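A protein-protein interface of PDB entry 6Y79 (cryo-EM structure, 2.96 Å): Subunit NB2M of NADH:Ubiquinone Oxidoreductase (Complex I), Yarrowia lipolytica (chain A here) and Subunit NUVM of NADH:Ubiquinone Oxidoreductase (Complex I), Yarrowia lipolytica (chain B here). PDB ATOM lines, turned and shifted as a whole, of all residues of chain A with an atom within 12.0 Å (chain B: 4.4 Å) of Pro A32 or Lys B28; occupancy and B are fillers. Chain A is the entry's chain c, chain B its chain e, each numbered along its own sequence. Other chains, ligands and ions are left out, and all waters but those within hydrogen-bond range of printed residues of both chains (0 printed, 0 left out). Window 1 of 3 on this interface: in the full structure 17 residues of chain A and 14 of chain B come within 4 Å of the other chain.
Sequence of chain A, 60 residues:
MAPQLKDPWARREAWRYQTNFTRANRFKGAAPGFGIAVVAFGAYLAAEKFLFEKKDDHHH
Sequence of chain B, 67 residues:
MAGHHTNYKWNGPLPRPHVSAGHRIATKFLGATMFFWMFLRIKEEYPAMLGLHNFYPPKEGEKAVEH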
ATOM      1  N   ASN A  25     -14.910 -13.570  -2.236  1.00  0.00           N
ATOM      2  CA  ASN A  25     -16.118 -12.903  -1.768  1.00  0.00           C
ATOM      3  C   ASN A  25     -17.137 -12.663  -2.870  1.00  0.00           C
ATOM      4  O   ASN A  25     -18.335 -12.579  -2.576  1.00  0.00           O
ATOM      5  CB  ASN A  25     -15.777 -11.555  -1.134  1.00  0.00           C
ATOM      6  CG  ASN A  25     -15.448 -11.667   0.332  1.00  0.00           C
ATOM      7  OD1 ASN A  25     -14.319 -11.414   0.734  1.00  0.00           O
ATOM      8  ND2 ASN A  25     -16.439 -12.018   1.145  1.00  0.00           N
ATOM      9  N   ARG A  26     -16.684 -12.514  -4.121  1.00  0.00           N
ATOM     10  CA  ARG A  26     -17.598 -12.206  -5.217  1.00  0.00           C
ATOM     11  C   ARG A  26     -18.569 -13.348  -5.486  1.00  0.00           C
ATOM     12  O   ARG A  26     -19.679 -13.111  -5.969  1.00  0.00           O
ATOM     13  CB  ARG A  26     -16.821 -11.867  -6.492  1.00  0.00           C
ATOM     14  CG  ARG A  26     -16.285 -10.437  -6.582  1.00  0.00           C
ATOM     15  CD  ARG A  26     -15.496 -10.237  -7.875  1.00  0.00           C
ATOM     16  NE  ARG A  26     -14.503 -11.288  -8.072  1.00  0.00           N
ATOM     17  CZ  ARG A  26     -13.729 -11.390  -9.145  1.00  0.00           C
ATOM     18  NH1 ARG A  26     -12.852 -12.382  -9.249  1.00  0.00           N
ATOM     19  NH2 ARG A  26     -13.832 -10.498 -10.114  1.00  0.00           N
ATOM     20  N   PHE A  27     -18.163 -14.589  -5.229  1.00  0.00           N
ATOM     21  CA  PHE A  27     -19.095 -15.717  -5.236  1.00  0.00           C
ATOM     22  C   PHE A  27     -19.405 -16.160  -3.806  1.00  0.00           C
ATOM     23  O   PHE A  27     -18.928 -17.191  -3.334  1.00  0.00           O
ATOM     24  CB  PHE A  27     -18.524 -16.881  -6.039  1.00  0.00           C
ATOM     25  CG  PHE A  27     -18.344 -16.605  -7.502  1.00  0.00           C
ATOM     26  CD1 PHE A  27     -19.032 -15.585  -8.139  1.00  0.00           C
ATOM     27  CD2 PHE A  27     -17.483 -17.397  -8.246  1.00  0.00           C
ATOM     28  CE1 PHE A  27     -18.853 -15.348  -9.482  1.00  0.00           C
ATOM     29  CE2 PHE A  27     -17.301 -17.171  -9.592  1.00  0.00           C
ATOM     30  CZ  PHE A  27     -17.989 -16.140 -10.211  1.00  0.00           C
ATOM     31  N   LYS A  28     -20.217 -15.383  -3.099  1.00  0.00           N
ATOM     32  CA  LYS A  28     -20.655 -15.866  -1.793  1.00  0.00           C
ATOM     33  C   LYS A  28     -22.165 -15.863  -1.630  1.00  0.00           C
ATOM     34  O   LYS A  28     -22.725 -16.817  -1.074  1.00  0.00           O
ATOM     35  CB  LYS A  28     -19.976 -15.077  -0.667  1.00  0.00           C
ATOM     36  CG  LYS A  28     -18.613 -15.665  -0.352  1.00  0.00           C
ATOM     37  CD  LYS A  28     -17.932 -15.034   0.840  1.00  0.00           C
ATOM     38  CE  LYS A  28     -16.514 -15.589   0.960  1.00  0.00           C
ATOM     39  NZ  LYS A  28     -15.680 -14.925   1.998  1.00  0.00           N
ATOM     40  N   GLY A  29     -22.847 -14.832  -2.107  1.00  0.00           N
ATOM     41  CA  GLY A  29     -24.292 -14.834  -2.048  1.00  0.00           C
ATOM     42  C   GLY A  29     -24.950 -15.434  -3.272  1.00  0.00           C
ATOM     43  O   GLY A  29     -26.161 -15.290  -3.440  1.00  0.00           O
ATOM     44  N   ALA A  30     -24.176 -16.129  -4.113  1.00  0.00           N
ATOM     45  CA  ALA A  30     -24.671 -16.543  -5.425  1.00  0.00           C
ATOM     46  C   ALA A  30     -25.722 -17.643  -5.316  1.00  0.00           C
ATOM     47  O   ALA A  30     -26.614 -17.742  -6.166  1.00  0.00           O
ATOM     48  CB  ALA A  30     -23.507 -16.994  -6.303  1.00  0.00           C
ATOM     49  N   ALA A  31     -25.637 -18.474  -4.283  1.00  0.00           N
ATOM     50  CA  ALA A  31     -26.646 -19.492  -3.995  1.00  0.00           C
ATOM     51  C   ALA A  31     -26.912 -19.453  -2.498  1.00  0.00           C
ATOM     52  O   ALA A  31     -26.386 -20.280  -1.742  1.00  0.00           O
ATOM     53  CB  ALA A  31     -26.190 -20.877  -4.453  1.00  0.00           C
ATOM     54  N   PRO A  32     -27.733 -18.503  -2.034  1.00  0.00           N
ATOM     55  CA  PRO A  32     -27.839 -18.251  -0.590  1.00  0.00           C
ATOM     56  C   PRO A  32     -28.611 -19.312   0.178  1.00  0.00           C
ATOM     57  O   PRO A  32     -28.286 -19.605   1.332  1.00  0.00           O
ATOM     58  CB  PRO A  32     -28.554 -16.898  -0.528  1.00  0.00           C
ATOM     59  CG  PRO A  32     -29.333 -16.832  -1.775  1.00  0.00           C
ATOM     60  CD  PRO A  32     -28.546 -17.558  -2.818  1.00  0.00           C
ATOM     61  N   GLY A  33     -29.625 -19.900  -0.440  1.00  0.00           N
ATOM     62  CA  GLY A  33     -30.411 -20.891   0.259  1.00  0.00           C
ATOM     63  C   GLY A  33     -30.162 -22.302  -0.216  1.00  0.00           C
ATOM     64  O   GLY A  33     -30.992 -23.181   0.009  1.00  0.00           O
ATOM     65  N   PHE A  34     -29.028 -22.531  -0.878  1.00  0.00           N
ATOM     66  CA  PHE A  34     -28.701 -23.873  -1.349  1.00  0.00           C
ATOM     67  C   PHE A  34     -28.410 -24.810  -0.183  1.00  0.00           C
ATOM     68  O   PHE A  34     -28.867 -25.960  -0.173  1.00  0.00           O
ATOM     69  CB  PHE A  34     -27.512 -23.797  -2.309  1.00  0.00           C
ATOM     70  CG  PHE A  34     -27.109 -25.116  -2.901  1.00  0.00           C
ATOM     71  CD1 PHE A  34     -27.825 -25.671  -3.948  1.00  0.00           C
ATOM     72  CD2 PHE A  34     -25.997 -25.786  -2.423  1.00  0.00           C
ATOM     73  CE1 PHE A  34     -27.444 -26.883  -4.496  1.00  0.00           C
ATOM     74  CE2 PHE A  34     -25.612 -26.995  -2.962  1.00  0.00           C
ATOM     75  CZ  PHE A  34     -26.336 -27.544  -4.002  1.00  0.00           C
ATOM     76  N   GLY A  35     -27.696 -24.315   0.830  1.00  0.00           N
ATOM     77  CA  GLY A  35     -27.275 -25.162   1.931  1.00  0.00           C
ATOM     78  C   GLY A  35     -28.395 -25.572   2.867  1.00  0.00           C
ATOM     79  O   GLY A  35     -28.306 -26.614   3.521  1.00  0.00           O
ATOM     80  N   ILE A  36     -29.443 -24.761   2.972  1.00  0.00           N
ATOM     81  CA  ILE A  36     -30.583 -25.191   3.772  1.00  0.00           C
ATOM     82  C   ILE A  36     -31.499 -26.080   2.946  1.00  0.00           C
ATOM     83  O   ILE A  36     -32.101 -27.029   3.463  1.00  0.00           O
ATOM     84  CB  ILE A  36     -31.321 -23.968   4.346  1.00  0.00           C
ATOM     85  CG1 ILE A  36     -30.329 -23.047   5.054  1.00  0.00           C
ATOM     86  CG2 ILE A  36     -32.410 -24.397   5.318  1.00  0.00           C
ATOM     87  CD1 ILE A  36     -30.939 -21.759   5.563  1.00  0.00           C
ATOM     88  N   ALA A  37     -31.585 -25.815   1.641  1.00  0.00           N
ATOM     89  CA  ALA A  37     -32.487 -26.584   0.799  1.00  0.00           C
ATOM     90  C   ALA A  37     -31.966 -27.985   0.536  1.00  0.00           C
ATOM     91  O   ALA A  37     -32.770 -28.891   0.309  1.00  0.00           O
ATOM     92  CB  ALA A  37     -32.735 -25.871  -0.523  1.00  0.00           C
ATOM     93  N   VAL A  38     -30.646 -28.198   0.581  1.00  0.00           N
ATOM     94  CA  VAL A  38     -30.159 -29.560   0.377  1.00  0.00           C
ATOM     95  C   VAL A  38     -30.518 -30.448   1.564  1.00  0.00           C
ATOM     96  O   VAL A  38     -30.922 -31.601   1.382  1.00  0.00           O
ATOM     97  CB  VAL A  38     -28.645 -29.586   0.075  1.00  0.00           C
ATOM     98  CG1 VAL A  38     -28.376 -29.046  -1.322  1.00  0.00           C
ATOM     99  CG2 VAL A  38     -27.836 -28.822   1.111  1.00  0.00           C
ATOM    100  N   VAL A  39     -30.477 -29.910   2.783  1.00  0.00           N
ATOM    101  CA  VAL A  39     -30.809 -30.721   3.948  1.00  0.00           C
ATOM    102  C   VAL A  39     -32.325 -30.818   4.119  1.00  0.00           C
ATOM    103  O   VAL A  39     -32.842 -31.851   4.558  1.00  0.00           O
ATOM    104  CB  VAL A  39     -30.091 -30.160   5.193  1.00  0.00           C
ATOM    105  CG1 VAL A  39     -30.425 -30.941   6.453  1.00  0.00           C
ATOM    106  CG2 VAL A  39     -28.594 -30.201   4.965  1.00  0.00           C
ATOM    107  N   ALA A  40     -33.070 -29.776   3.720  1.00  0.00           N
ATOM    108  CA  ALA A  40     -34.529 -29.881   3.708  1.00  0.00           C
ATOM    109  C   ALA A  40     -35.010 -30.883   2.667  1.00  0.00           C
ATOM    110  O   ALA A  40     -35.963 -31.633   2.916  1.00  0.00           O
ATOM    111  CB  ALA A  40     -35.157 -28.516   3.453  1.00  0.00           C
ATOM    112  N   ARG B  24     -31.402  -9.995   5.710  1.00  0.00           N
ATOM    113  CA  ARG B  24     -30.528 -11.164   5.616  1.00  0.00           C
ATOM    114  C   ARG B  24     -31.269 -12.473   5.900  1.00  0.00           C
ATOM    115  O   ARG B  24     -30.934 -13.511   5.319  1.00  0.00           O
ATOM    116  CB  ARG B  24     -29.348 -10.975   6.574  1.00  0.00           C
ATOM    117  CG  ARG B  24     -28.292 -12.068   6.586  1.00  0.00           C
ATOM    118  CD  ARG B  24     -27.770 -12.403   5.192  1.00  0.00           C
ATOM    119  NE  ARG B  24     -27.107 -11.288   4.517  1.00  0.00           N
ATOM    120  CZ  ARG B  24     -25.850 -10.914   4.735  1.00  0.00           C
ATOM    121  NH1 ARG B  24     -25.104 -11.553   5.628  1.00  0.00           N
ATOM    122  NH2 ARG B  24     -25.333  -9.898   4.057  1.00  0.00           N
ATOM    123  N   ILE B  25     -32.290 -12.442   6.761  1.00  0.00           N
ATOM    124  CA  ILE B  25     -33.131 -13.619   6.977  1.00  0.00           C
ATOM    125  C   ILE B  25     -34.053 -13.851   5.781  1.00  0.00           C
ATOM    126  O   ILE B  25     -34.235 -15.004   5.344  1.00  0.00           O
ATOM    127  CB  ILE B  25     -33.936 -13.486   8.288  1.00  0.00           C
ATOM    128  CG1 ILE B  25     -33.012 -13.428   9.509  1.00  0.00           C
ATOM    129  CG2 ILE B  25     -34.949 -14.608   8.450  1.00  0.00           C
ATOM    130  CD1 ILE B  25     -32.067 -14.612   9.657  1.00  0.00           C
ATOM    131  N   ALA B  26     -34.614 -12.772   5.217  1.00  0.00           N
ATOM    132  CA  ALA B  26     -35.593 -12.898   4.140  1.00  0.00           C
ATOM    133  C   ALA B  26     -34.988 -13.488   2.868  1.00  0.00           C
ATOM    134  O   ALA B  26     -35.660 -14.258   2.167  1.00  0.00           O
ATOM    135  CB  ALA B  26     -36.206 -11.530   3.840  1.00  0.00           C
ATOM    136  N   THR B  27     -33.718 -13.178   2.576  1.00  0.00           N
ATOM    137  CA  THR B  27     -33.106 -13.712   1.353  1.00  0.00           C
ATOM    138  C   THR B  27     -32.769 -15.187   1.491  1.00  0.00           C
ATOM    139  O   THR B  27     -32.832 -15.938   0.511  1.00  0.00           O
ATOM    140  CB  THR B  27     -31.845 -12.950   0.973  1.00  0.00           C
ATOM    141  OG1 THR B  27     -30.762 -13.342   1.807  1.00  0.00           O
ATOM    142  CG2 THR B  27     -32.061 -11.542   1.129  1.00  0.00           C
ATOM    143  N   LYS B  28     -32.343 -15.603   2.687  1.00  0.00           N
ATOM    144  CA  LYS B  28     -32.092 -17.020   2.919  1.00  0.00           C
ATOM    145  C   LYS B  28     -33.384 -17.819   2.874  1.00  0.00           C
ATOM    146  O   LYS B  28     -33.394 -18.956   2.385  1.00  0.00           O
ATOM    147  CB  LYS B  28     -31.363 -17.224   4.240  1.00  0.00           C
ATOM    148  CG  LYS B  28     -29.894 -16.842   4.163  1.00  0.00           C
ATOM    149  CD  LYS B  28     -29.151 -17.107   5.455  1.00  0.00           C
ATOM    150  CE  LYS B  28     -28.892 -18.594   5.655  1.00  0.00           C
ATOM    151  NZ  LYS B  28     -27.883 -19.121   4.691  1.00  0.00           N
ATOM    152  N   PHE B  29     -34.497 -17.208   3.302  1.00  0.00           N
ATOM    153  CA  PHE B  29     -35.796 -17.854   3.137  1.00  0.00           C
ATOM    154  C   PHE B  29     -36.175 -17.991   1.663  1.00  0.00           C
ATOM    155  O   PHE B  29     -36.620 -19.062   1.230  1.00  0.00           O
ATOM    156  CB  PHE B  29     -36.878 -17.090   3.892  1.00  0.00           C
ATOM    157  CG  PHE B  29     -38.235 -17.733   3.791  1.00  0.00           C
ATOM    158  CD1 PHE B  29     -38.504 -18.906   4.472  1.00  0.00           C
ATOM    159  CD2 PHE B  29     -39.234 -17.175   3.005  1.00  0.00           C
ATOM    160  CE1 PHE B  29     -39.743 -19.511   4.382  1.00  0.00           C
ATOM    161  CE2 PHE B  29     -40.477 -17.775   2.907  1.00  0.00           C
ATOM    162  CZ  PHE B  29     -40.731 -18.944   3.599  1.00  0.00           C
ATOM    163  N   LEU B  30     -35.998 -16.920   0.874  1.00  0.00           N
ATOM    164  CA  LEU B  30     -36.377 -16.970  -0.540  1.00  0.00           C
ATOM    165  C   LEU B  30     -35.493 -17.928  -1.337  1.00  0.00           C
ATOM    166  O   LEU B  30     -35.991 -18.692  -2.177  1.00  0.00           O
ATOM    167  CB  LEU B  30     -36.329 -15.571  -1.154  1.00  0.00           C
ATOM    168  CG  LEU B  30     -37.511 -14.655  -0.845  1.00  0.00           C
ATOM    169  CD1 LEU B  30     -37.334 -13.299  -1.503  1.00  0.00           C
ATOM    170  CD2 LEU B  30     -38.803 -15.298  -1.295  1.00  0.00           C
ATOM    171  N   GLY B  31     -34.186 -17.922  -1.068  1.00  0.00           N
ATOM    172  CA  GLY B  31     -33.291 -18.837  -1.756  1.00  0.00           C
ATOM    173  C   GLY B  31     -33.498 -20.286  -1.356  1.00  0.00           C
ATOM    174  O   GLY B  31     -33.428 -21.191  -2.195  1.00  0.00           O
ATOM    175  N   ALA B  32     -33.755 -20.536  -0.070  1.00  0.00           N
ATOM    176  CA  ALA B  32     -34.040 -21.895   0.365  1.00  0.00           C
ATOM    177  C   ALA B  32     -35.338 -22.402  -0.248  1.00  0.00           C
ATOM    178  O   ALA B  32     -35.410 -23.558  -0.686  1.00  0.00           O
ATOM    179  CB  ALA B  32     -34.096 -21.951   1.888  1.00  0.00           C
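The side-chain amino group (NZ) of Lys B28 sits at hydrogen-bond distance from the backbone carbonyl oxygen (O) of Pro A32 (3.4 Å).
Gly A33 touches Gly B31. Gly A33 touches Ala B32. Ile A36 touches Lys B28. Ala B32 touches Ala A37 (O to CB, 3.5 Å).
Of the printed residues of chain B, Pro A32 touches Lys B28 (3.4 Å). Of the printed residues of chain A, Lys B28 touches Pro A32 (3.4 Å) and Ile A36 (3.8 Å). No residue of chain A comes within 4 Å of Ile B25. No residue of chain A comes within 4 Å of Ala B26. No residue of chain A comes within 4 Å of Thr B27. No residue of chain A comes within 4 Å of Phe B29. Of the printed residues of chain A, Ala B32 touches Gly A33 (3.3 Å) and Ala A37 (3.5 Å). Of the printed residues of chain B, Ile A36 touches Lys B28. Of the printed residues of chain B, Ala A37 touches Ala B32. Ala A30 touches none of the printed residues of chain B. The nearest residue of chain B that does not touch Pro A32 is Thr B27 (4.3 Å).
Of the 9 printed residues of chain B, 3 touch a printed residue of chain A. Hydrophobic or aromatic side chains of chain B within 4 Å of the printed part of chain A: Ala B32. Of the 16 printed residues of chain A, 4 touch a printed residue of chain B. Hydrophobic or aromatic side chains of chain A within 4 Å of the printed part of chain B: Ile A36 and Ala A37. Among the printed residues, 5 pairs touch across the chains.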
